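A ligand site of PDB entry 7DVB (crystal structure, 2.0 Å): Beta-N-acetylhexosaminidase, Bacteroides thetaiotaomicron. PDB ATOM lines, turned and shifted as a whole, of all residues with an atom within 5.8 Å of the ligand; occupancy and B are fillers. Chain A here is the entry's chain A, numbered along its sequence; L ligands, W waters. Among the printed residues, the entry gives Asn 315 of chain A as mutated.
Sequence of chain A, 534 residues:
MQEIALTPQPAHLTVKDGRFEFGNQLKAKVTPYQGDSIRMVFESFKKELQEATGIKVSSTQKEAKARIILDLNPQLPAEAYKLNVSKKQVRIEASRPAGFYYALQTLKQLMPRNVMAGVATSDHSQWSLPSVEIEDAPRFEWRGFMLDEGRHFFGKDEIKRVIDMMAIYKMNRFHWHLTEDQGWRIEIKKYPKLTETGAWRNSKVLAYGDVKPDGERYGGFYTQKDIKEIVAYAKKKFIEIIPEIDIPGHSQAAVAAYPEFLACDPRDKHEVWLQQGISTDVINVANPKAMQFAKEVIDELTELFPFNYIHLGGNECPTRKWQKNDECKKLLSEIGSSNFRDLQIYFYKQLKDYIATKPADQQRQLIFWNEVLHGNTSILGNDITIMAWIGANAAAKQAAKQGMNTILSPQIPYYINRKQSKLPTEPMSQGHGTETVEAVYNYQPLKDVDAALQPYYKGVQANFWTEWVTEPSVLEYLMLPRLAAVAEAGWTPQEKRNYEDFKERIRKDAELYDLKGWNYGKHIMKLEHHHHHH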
ATOM      1  N   ASP A 148       5.557  18.790 -23.314  1.00  0.00           N
ATOM      2  CA  ASP A 148       4.785  19.646 -22.434  1.00  0.00           C
ATOM      3  C   ASP A 148       3.367  19.744 -22.987  1.00  0.00           C
ATOM      4  O   ASP A 148       3.158  20.336 -24.043  1.00  0.00           O
ATOM      5  CB  ASP A 148       5.453  21.028 -22.343  1.00  0.00           C
ATOM      6  CG  ASP A 148       4.578  22.132 -21.788  1.00  0.00           C
ATOM      7  OD1 ASP A 148       3.579  21.826 -21.080  1.00  0.00           O
ATOM      8  OD2 ASP A 148       4.911  23.313 -22.051  1.00  0.00           O
ATOM      9  N   ARG A 151       0.978  23.510 -21.297  1.00  0.00           N
ATOM     10  CA  ARG A 151       0.805  24.783 -22.002  1.00  0.00           C
ATOM     11  C   ARG A 151      -0.232  24.640 -23.117  1.00  0.00           C
ATOM     12  O   ARG A 151      -1.153  25.443 -23.203  1.00  0.00           O
ATOM     13  CB  ARG A 151       2.155  25.328 -22.476  1.00  0.00           C
ATOM     14  CG  ARG A 151       2.922  26.134 -21.430  1.00  0.00           C
ATOM     15  CD  ARG A 151       3.253  25.386 -20.163  1.00  0.00           C
ATOM     16  NE  ARG A 151       4.131  26.125 -19.255  1.00  0.00           N
ATOM     17  CZ  ARG A 151       5.468  26.110 -19.292  1.00  0.00           C
ATOM     18  NH1 ARG A 151       6.097  25.380 -20.199  1.00  0.00           N
ATOM     19  NH2 ARG A 151       6.163  26.829 -18.423  1.00  0.00           N
ATOM     20  N   GLU A 180       1.066  21.986 -15.088  1.00  0.00           N
ATOM     21  CA  GLU A 180       1.643  23.310 -15.287  1.00  0.00           C
ATOM     22  C   GLU A 180       0.835  24.394 -14.584  1.00  0.00           C
ATOM     23  O   GLU A 180      -0.209  24.123 -13.992  1.00  0.00           O
ATOM     24  CB  GLU A 180       1.761  23.612 -16.783  1.00  0.00           C
ATOM     25  CG  GLU A 180       3.106  23.236 -17.361  1.00  0.00           C
ATOM     26  CD  GLU A 180       4.282  24.026 -16.790  1.00  0.00           C
ATOM     27  OE1 GLU A 180       4.045  25.096 -16.196  1.00  0.00           O
ATOM     28  OE2 GLU A 180       5.430  23.573 -16.950  1.00  0.00           O
ATOM     29  N   HIS A 250       5.445  25.623 -10.654  1.00  0.00           N
ATOM     30  CA  HIS A 250       4.740  25.341 -11.894  1.00  0.00           C
ATOM     31  C   HIS A 250       3.412  24.642 -11.599  1.00  0.00           C
ATOM     32  O   HIS A 250       3.017  23.737 -12.329  1.00  0.00           O
ATOM     33  CB  HIS A 250       5.630  24.541 -12.859  1.00  0.00           C
ATOM     34  CG  HIS A 250       6.580  25.392 -13.633  1.00  0.00           C
ATOM     35  ND1 HIS A 250       6.203  26.071 -14.766  1.00  0.00           N
ATOM     36  CD2 HIS A 250       7.875  25.690 -13.435  1.00  0.00           C
ATOM     37  CE1 HIS A 250       7.226  26.754 -15.242  1.00  0.00           C
ATOM     38  NE2 HIS A 250       8.266  26.533 -14.437  1.00  0.00           N
ATOM     39  N   GLY A 277       5.688  32.420 -18.535  1.00  0.00           N
ATOM     40  CA  GLY A 277       6.650  32.928 -17.561  1.00  0.00           C
ATOM     41  C   GLY A 277       6.773  32.011 -16.342  1.00  0.00           C
ATOM     42  O   GLY A 277       6.534  30.811 -16.429  1.00  0.00           O
ATOM     43  N   ASN A 315      11.667  22.712 -10.988  1.00  0.00           N
ATOM     44  CA  ASN A 315      12.223  23.828 -11.737  1.00  0.00           C
ATOM     45  C   ASN A 315      11.522  25.114 -11.312  1.00  0.00           C
ATOM     46  O   ASN A 315      10.355  25.087 -10.930  1.00  0.00           O
ATOM     47  CB  ASN A 315      12.082  23.636 -13.248  1.00  0.00           C
ATOM     48  CG  ASN A 315      10.647  23.407 -13.683  1.00  0.00           C
ATOM     49  OD1 ASN A 315       9.888  22.692 -13.025  1.00  0.00           O
ATOM     50  ND2 ASN A 315      10.249  24.007 -14.796  1.00  0.00           N
ATOM     51  N   GLU A 316      12.262  26.225 -11.383  1.00  0.00           N
ATOM     52  CA  GLU A 316      11.732  27.581 -11.344  1.00  0.00           C
ATOM     53  C   GLU A 316      10.657  27.691 -10.282  1.00  0.00           C
ATOM     54  O   GLU A 316       9.485  27.939 -10.580  1.00  0.00           O
ATOM     55  CB  GLU A 316      11.143  27.959 -12.701  1.00  0.00           C
ATOM     56  CG  GLU A 316      12.144  27.964 -13.846  1.00  0.00           C
ATOM     57  CD  GLU A 316      11.525  28.274 -15.206  1.00  0.00           C
ATOM     58  OE1 GLU A 316      10.311  28.054 -15.383  1.00  0.00           O
ATOM     59  OE2 GLU A 316      12.285  28.724 -16.086  1.00  0.00           O
ATOM     60  N   TRP A 369      14.495  18.356 -11.898  1.00  0.00           N
ATOM     61  CA  TRP A 369      15.249  19.355 -12.636  1.00  0.00           C
ATOM     62  C   TRP A 369      16.373  19.866 -11.730  1.00  0.00           C
ATOM     63  O   TRP A 369      16.239  19.862 -10.502  1.00  0.00           O
ATOM     64  CB  TRP A 369      14.346  20.493 -13.101  1.00  0.00           C
ATOM     65  CG  TRP A 369      13.197  20.101 -13.992  1.00  0.00           C
ATOM     66  CD1 TRP A 369      11.882  20.109 -13.662  1.00  0.00           C
ATOM     67  CD2 TRP A 369      13.259  19.686 -15.370  1.00  0.00           C
ATOM     68  NE1 TRP A 369      11.111  19.715 -14.730  1.00  0.00           N
ATOM     69  CE2 TRP A 369      11.939  19.456 -15.792  1.00  0.00           C
ATOM     70  CE3 TRP A 369      14.295  19.509 -16.291  1.00  0.00           C
ATOM     71  CZ2 TRP A 369      11.619  19.038 -17.093  1.00  0.00           C
ATOM     72  CZ3 TRP A 369      13.980  19.093 -17.568  1.00  0.00           C
ATOM     73  CH2 TRP A 369      12.652  18.868 -17.968  1.00  0.00           C
ATOM     74  N   GLU A 371      17.631  22.489 -10.588  1.00  0.00           N
ATOM     75  CA  GLU A 371      17.562  23.562  -9.602  1.00  0.00           C
ATOM     76  C   GLU A 371      17.514  22.992  -8.175  1.00  0.00           C
ATOM     77  O   GLU A 371      17.788  23.703  -7.215  1.00  0.00           O
ATOM     78  CB  GLU A 371      16.369  24.486  -9.817  1.00  0.00           C
ATOM     79  CG  GLU A 371      16.472  25.360 -11.050  1.00  0.00           C
ATOM     80  CD  GLU A 371      15.621  24.866 -12.209  1.00  0.00           C
ATOM     81  OE1 GLU A 371      15.666  23.651 -12.501  1.00  0.00           O
ATOM     82  OE2 GLU A 371      14.889  25.683 -12.772  1.00  0.00           O
ATOM     83  N   TRP A 389      19.315  20.879 -17.242  1.00  0.00           N
ATOM     84  CA  TRP A 389      18.757  21.690 -18.319  1.00  0.00           C
ATOM     85  C   TRP A 389      19.393  23.080 -18.378  1.00  0.00           C
ATOM     86  O   TRP A 389      19.664  23.589 -19.465  1.00  0.00           O
ATOM     87  CB  TRP A 389      17.226  21.772 -18.235  1.00  0.00           C
ATOM     88  CG  TRP A 389      16.687  22.747 -17.240  1.00  0.00           C
ATOM     89  CD1 TRP A 389      16.387  22.510 -15.934  1.00  0.00           C
ATOM     90  CD2 TRP A 389      16.378  24.140 -17.467  1.00  0.00           C
ATOM     91  NE1 TRP A 389      15.909  23.639 -15.344  1.00  0.00           N
ATOM     92  CE2 TRP A 389      15.899  24.659 -16.252  1.00  0.00           C
ATOM     93  CE3 TRP A 389      16.478  24.995 -18.584  1.00  0.00           C
ATOM     94  CZ2 TRP A 389      15.505  25.993 -16.111  1.00  0.00           C
ATOM     95  CZ3 TRP A 389      16.097  26.318 -18.452  1.00  0.00           C
ATOM     96  CH2 TRP A 389      15.624  26.801 -17.232  1.00  0.00           C
ATOM     97  N   GLN A 411      19.015  23.281 -22.379  1.00  0.00           N
ATOM     98  CA  GLN A 411      18.179  24.239 -23.093  1.00  0.00           C
ATOM     99  C   GLN A 411      18.720  24.450 -24.511  1.00  0.00           C
ATOM    100  O   GLN A 411      17.973  24.341 -25.482  1.00  0.00           O
ATOM    101  CB  GLN A 411      18.087  25.551 -22.317  1.00  0.00           C
ATOM    102  CG  GLN A 411      17.336  26.638 -23.061  1.00  0.00           C
ATOM    103  CD  GLN A 411      17.069  27.805 -22.139  1.00  0.00           C
ATOM    104  OE1 GLN A 411      17.969  28.329 -21.479  1.00  0.00           O
ATOM    105  NE2 GLN A 411      15.820  28.231 -22.101  1.00  0.00           N
ATOM    106  N   TYR A 415      16.410  21.769 -26.525  1.00  0.00           N
ATOM    107  CA  TYR A 415      15.023  22.227 -26.504  1.00  0.00           C
ATOM    108  C   TYR A 415      14.553  22.380 -27.952  1.00  0.00           C
ATOM    109  O   TYR A 415      14.749  23.427 -28.563  1.00  0.00           O
ATOM    110  CB  TYR A 415      14.896  23.507 -25.680  1.00  0.00           C
ATOM    111  CG  TYR A 415      14.866  23.336 -24.174  1.00  0.00           C
ATOM    112  CD1 TYR A 415      15.299  22.155 -23.583  1.00  0.00           C
ATOM    113  CD2 TYR A 415      14.446  24.365 -23.339  1.00  0.00           C
ATOM    114  CE1 TYR A 415      15.276  21.982 -22.203  1.00  0.00           C
ATOM    115  CE2 TYR A 415      14.414  24.211 -21.972  1.00  0.00           C
ATOM    116  CZ  TYR A 415      14.824  23.015 -21.396  1.00  0.00           C
ATOM    117  OH  TYR A 415      14.779  22.827 -20.048  1.00  0.00           O
ATOM    118  N   ASN A 417      11.722  22.658 -29.320  1.00  0.00           N
ATOM    119  CA  ASN A 417      10.601  23.534 -29.625  1.00  0.00           C
ATOM    120  C   ASN A 417      11.144  24.868 -30.137  1.00  0.00           C
ATOM    121  O   ASN A 417      10.405  25.638 -30.736  1.00  0.00           O
ATOM    122  CB  ASN A 417       9.718  23.789 -28.413  1.00  0.00           C
ATOM    123  CG  ASN A 417      10.502  24.294 -27.232  1.00  0.00           C
ATOM    124  OD1 ASN A 417      11.187  23.517 -26.558  1.00  0.00           O
ATOM    125  ND2 ASN A 417      10.437  25.591 -26.977  1.00  0.00           N
ATOM    126  N   ARG A 418      12.434  25.136 -29.892  1.00  0.00           N
ATOM    127  CA  ARG A 418      13.077  26.385 -30.299  1.00  0.00           C
ATOM    128  C   ARG A 418      13.178  26.444 -31.828  1.00  0.00           C
ATOM    129  O   ARG A 418      13.227  25.411 -32.490  1.00  0.00           O
ATOM    130  CB  ARG A 418      14.430  26.545 -29.618  1.00  0.00           C
ATOM    131  CG  ARG A 418      14.364  26.696 -28.097  1.00  0.00           C
ATOM    132  CD  ARG A 418      15.727  26.733 -27.427  1.00  0.00           C
ATOM    133  NE  ARG A 418      16.481  27.929 -27.769  1.00  0.00           N
ATOM    134  CZ  ARG A 418      16.425  29.086 -27.112  1.00  0.00           C
ATOM    135  NH1 ARG A 418      15.670  29.198 -26.031  1.00  0.00           N
ATOM    136  NH2 ARG A 418      17.161  30.112 -27.510  1.00  0.00           N
ATOM    137  N   GLN A 430      10.242  29.920 -29.331  1.00  0.00           N
ATOM    138  CA  GLN A 430      11.355  30.562 -28.640  1.00  0.00           C
ATOM    139  C   GLN A 430      12.641  30.441 -29.457  1.00  0.00           C
ATOM    140  O   GLN A 430      12.760  29.557 -30.308  1.00  0.00           O
ATOM    141  CB  GLN A 430      11.544  29.951 -27.256  1.00  0.00           C
ATOM    142  CG  GLN A 430      10.342  30.108 -26.331  1.00  0.00           C
ATOM    143  CD  GLN A 430       9.410  28.921 -26.329  1.00  0.00           C
ATOM    144  OE1 GLN A 430       9.167  28.254 -27.337  1.00  0.00           O
ATOM    145  NE2 GLN A 430       8.836  28.655 -25.171  1.00  0.00           N
ATOM    146  N   ASN A 463      13.670  18.066 -25.206  1.00  0.00           N
ATOM    147  CA  ASN A 463      12.473  18.556 -24.541  1.00  0.00           C
ATOM    148  C   ASN A 463      11.705  19.469 -25.491  1.00  0.00           C
ATOM    149  O   ASN A 463      12.305  20.175 -26.307  1.00  0.00           O
ATOM    150  CB  ASN A 463      12.804  19.281 -23.226  1.00  0.00           C
ATOM    151  CG  ASN A 463      13.450  18.393 -22.185  1.00  0.00           C
ATOM    152  OD1 ASN A 463      13.469  17.174 -22.328  1.00  0.00           O
ATOM    153  ND2 ASN A 463      13.990  19.003 -21.142  1.00  0.00           N
ATOM    154  N   TRP A 465       8.710  22.321 -25.207  1.00  0.00           N
ATOM    155  CA  TRP A 465       7.868  23.204 -24.428  1.00  0.00           C
ATOM    156  C   TRP A 465       6.899  23.916 -25.363  1.00  0.00           C
ATOM    157  O   TRP A 465       7.279  24.309 -26.479  1.00  0.00           O
ATOM    158  CB  TRP A 465       8.762  24.195 -23.657  1.00  0.00           C
ATOM    159  CG  TRP A 465       9.774  23.502 -22.805  1.00  0.00           C
ATOM    160  CD1 TRP A 465      11.092  23.274 -23.106  1.00  0.00           C
ATOM    161  CD2 TRP A 465       9.546  22.902 -21.521  1.00  0.00           C
ATOM    162  NE1 TRP A 465      11.692  22.586 -22.087  1.00  0.00           N
ATOM    163  CE2 TRP A 465      10.776  22.336 -21.096  1.00  0.00           C
ATOM    164  CE3 TRP A 465       8.429  22.786 -20.681  1.00  0.00           C
ATOM    165  CZ2 TRP A 465      10.907  21.680 -19.876  1.00  0.00           C
ATOM    166  CZ3 TRP A 465       8.564  22.139 -19.465  1.00  0.00           C
ATOM    167  CH2 TRP A 465       9.796  21.602 -19.069  1.00  0.00           C
ATOM    168  N   THR A 466       5.645  24.087 -24.914  1.00  0.00           N
ATOM    169  CA  THR A 466       4.575  24.427 -25.850  1.00  0.00           C
ATOM    170  C   THR A 466       3.902  25.769 -25.549  1.00  0.00           C
ATOM    171  O   THR A 466       2.742  25.944 -25.910  1.00  0.00           O
ATOM    172  CB  THR A 466       3.560  23.285 -25.986  1.00  0.00           C
ATOM    173  OG1 THR A 466       2.960  23.029 -24.714  1.00  0.00           O
ATOM    174  CG2 THR A 466       4.158  22.023 -26.551  1.00  0.00           C
ATOM    175  N   GLU A 467       4.623  26.725 -24.943  1.00  0.00           N
ATOM    176  CA  GLU A 467       4.086  28.068 -24.743  1.00  0.00           C
ATOM    177  C   GLU A 467       3.467  28.602 -26.032  1.00  0.00           C
ATOM    178  O   GLU A 467       2.373  29.157 -26.011  1.00  0.00           O
ATOM    179  CB  GLU A 467       5.162  29.061 -24.287  1.00  0.00           C
ATOM    180  CG  GLU A 467       5.552  28.914 -22.830  1.00  0.00           C
ATOM    181  CD  GLU A 467       6.748  28.014 -22.597  1.00  0.00           C
ATOM    182  OE1 GLU A 467       6.940  27.065 -23.382  1.00  0.00           O
ATOM    183  OE2 GLU A 467       7.500  28.272 -21.625  1.00  0.00           O
HETATM  184  O1  LIG L   1      14.046  27.466 -24.601  1.00  0.00           O
HETATM  185  O2  LIG L   1      12.473  29.132 -23.833  1.00  0.00           O
HETATM  186  S1  LIG L   1      12.676  27.748 -24.189  1.00  0.00           S
HETATM  187  O3  LIG L   1      11.694  27.265 -25.137  1.00  0.00           O
HETATM  188  C1  LIG L   1      12.583  26.097 -18.885  1.00  0.00           C
HETATM  189  C2  LIG L   1      11.332  26.112 -18.007  1.00  0.00           C
HETATM  190  C3  LIG L   1      10.032  25.833 -18.764  1.00  0.00           C
HETATM  191  C4  LIG L   1       9.964  26.593 -20.075  1.00  0.00           C
HETATM  192  C5  LIG L   1      11.189  26.262 -20.917  1.00  0.00           C
HETATM  193  C6  LIG L   1      11.180  26.988 -22.234  1.00  0.00           C
HETATM  194  C7  LIG L   1      12.489  24.182 -17.668  1.00  0.00           C
HETATM  195  C8  LIG L   1      12.956  22.846 -17.179  1.00  0.00           C
HETATM  196  N1  LIG L   1      11.645  24.977 -17.111  1.00  0.00           N
HETATM  197  O4  LIG L   1      12.982  24.689 -18.840  1.00  0.00           O
HETATM  198  O5  LIG L   1       8.924  26.142 -17.903  1.00  0.00           O
HETATM  199  O6  LIG L   1       8.816  26.162 -20.804  1.00  0.00           O
HETATM  200  O7  LIG L   1      12.420  26.562 -20.215  1.00  0.00           O
HETATM  201  O8  LIG L   1      12.478  26.930 -22.845  1.00  0.00           O
HETATM  202  O   HOH W   1       8.067  23.896 -16.491  1.00  0.00           O
HETATM  203  O   HOH W   2       9.409  30.176 -22.713  1.00  0.00           O
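The side-chain carboxylate (OE2) of Glu 467 sits at hydrogen-bond distance from an oxygen (O6) of the ligand. The guanidinium group (NH1) of Arg 418 is in salt-bridge range of an oxygen (O1) of the ligand (2.8 Å). An oxygen (O3) of the ligand lies within hydrogen-bond range of the side-chain amide nitrogen (ND2) of Asn 417 (2.8 Å). The side-chain hydroxyl (OH) of Tyr 415 lies within hydrogen-bond range of an oxygen (O4) of the ligand, at 2.9 Å. The side-chain amide nitrogen (ND2) of Asn 315 sits close to a nitrogen (N1) of the ligand, 2.9 Å away. NH2 of Arg 151 is in hydrogen-bond range of O5 of the ligand (2.9 Å). The side-chain amide nitrogen of Gln 430 lies close to an oxygen (O3) of the ligand (3.2 Å). An oxygen (O1) of the ligand is in hydrogen-bond range of the side-chain amide nitrogen (NE2) of Gln 411. OE1 of Glu 316 is in salt-bridge range of N1 of the ligand (3.8 Å).
The side-chain amide nitrogen of Asn 417 sits at hydrogen-bond distance from the side-chain amide oxygen of Gln 430 (3.0 Å). The side-chain amide oxygen of Asn 417 lies within hydrogen-bond range of the backbone NH of Trp 465 (3.1 Å). The side-chain amide nitrogen of Asn 315 lies close to a ring nitrogen (NE2) of His 250, at 3.2 Å. The guanidinium group of Arg 151 is in salt-bridge range of the side-chain carboxylate of Glu 180 (3.2 Å). The side-chain carboxylate (OD2) of Asp 148 lies within salt-bridge range of the guanidinium group (NH1) of Arg 151 (3.0 Å). N of Gln 411 is in hydrogen-bond range of O of Trp 389 (3.0 Å). ND1 of His 250 is in hydrogen-bond range of OE1 of Glu 180 (2.8 Å). OE1 of Glu 371 is in hydrogen-bond range of NE1 of Trp 389.
Merely in contact with the ligand: His 250, Trp 369, Trp 389 and Trp 465. 13 residues have an atom within 4 Å of the ligand: Arg 151, His 250, Asn 315, Glu 316, Trp 369, Trp 389, Gln 411, Tyr 415, Asn 417, Arg 418, Gln 430, Trp 465 and Glu 467. The nearest printed residue that does not touch the ligand is Glu 180 (4.4 Å).
Water W1 lies within hydrogen-bond range of the side-chain carboxylate (OE2) of Glu 180 (2.7 Å), the side-chain amide nitrogen (ND2) of Asn 315 (2.8 Å), an oxygen (O5) of the ligand (2.8 Å) and a ring nitrogen (ND1) of His 250 (3.3 Å). Water W2 lies within hydrogen-bond range of OE2 of Glu 467 (2.9 Å), NE2 of Gln 430 (2.9 Å) and O2 of the ligand (3.4 Å).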
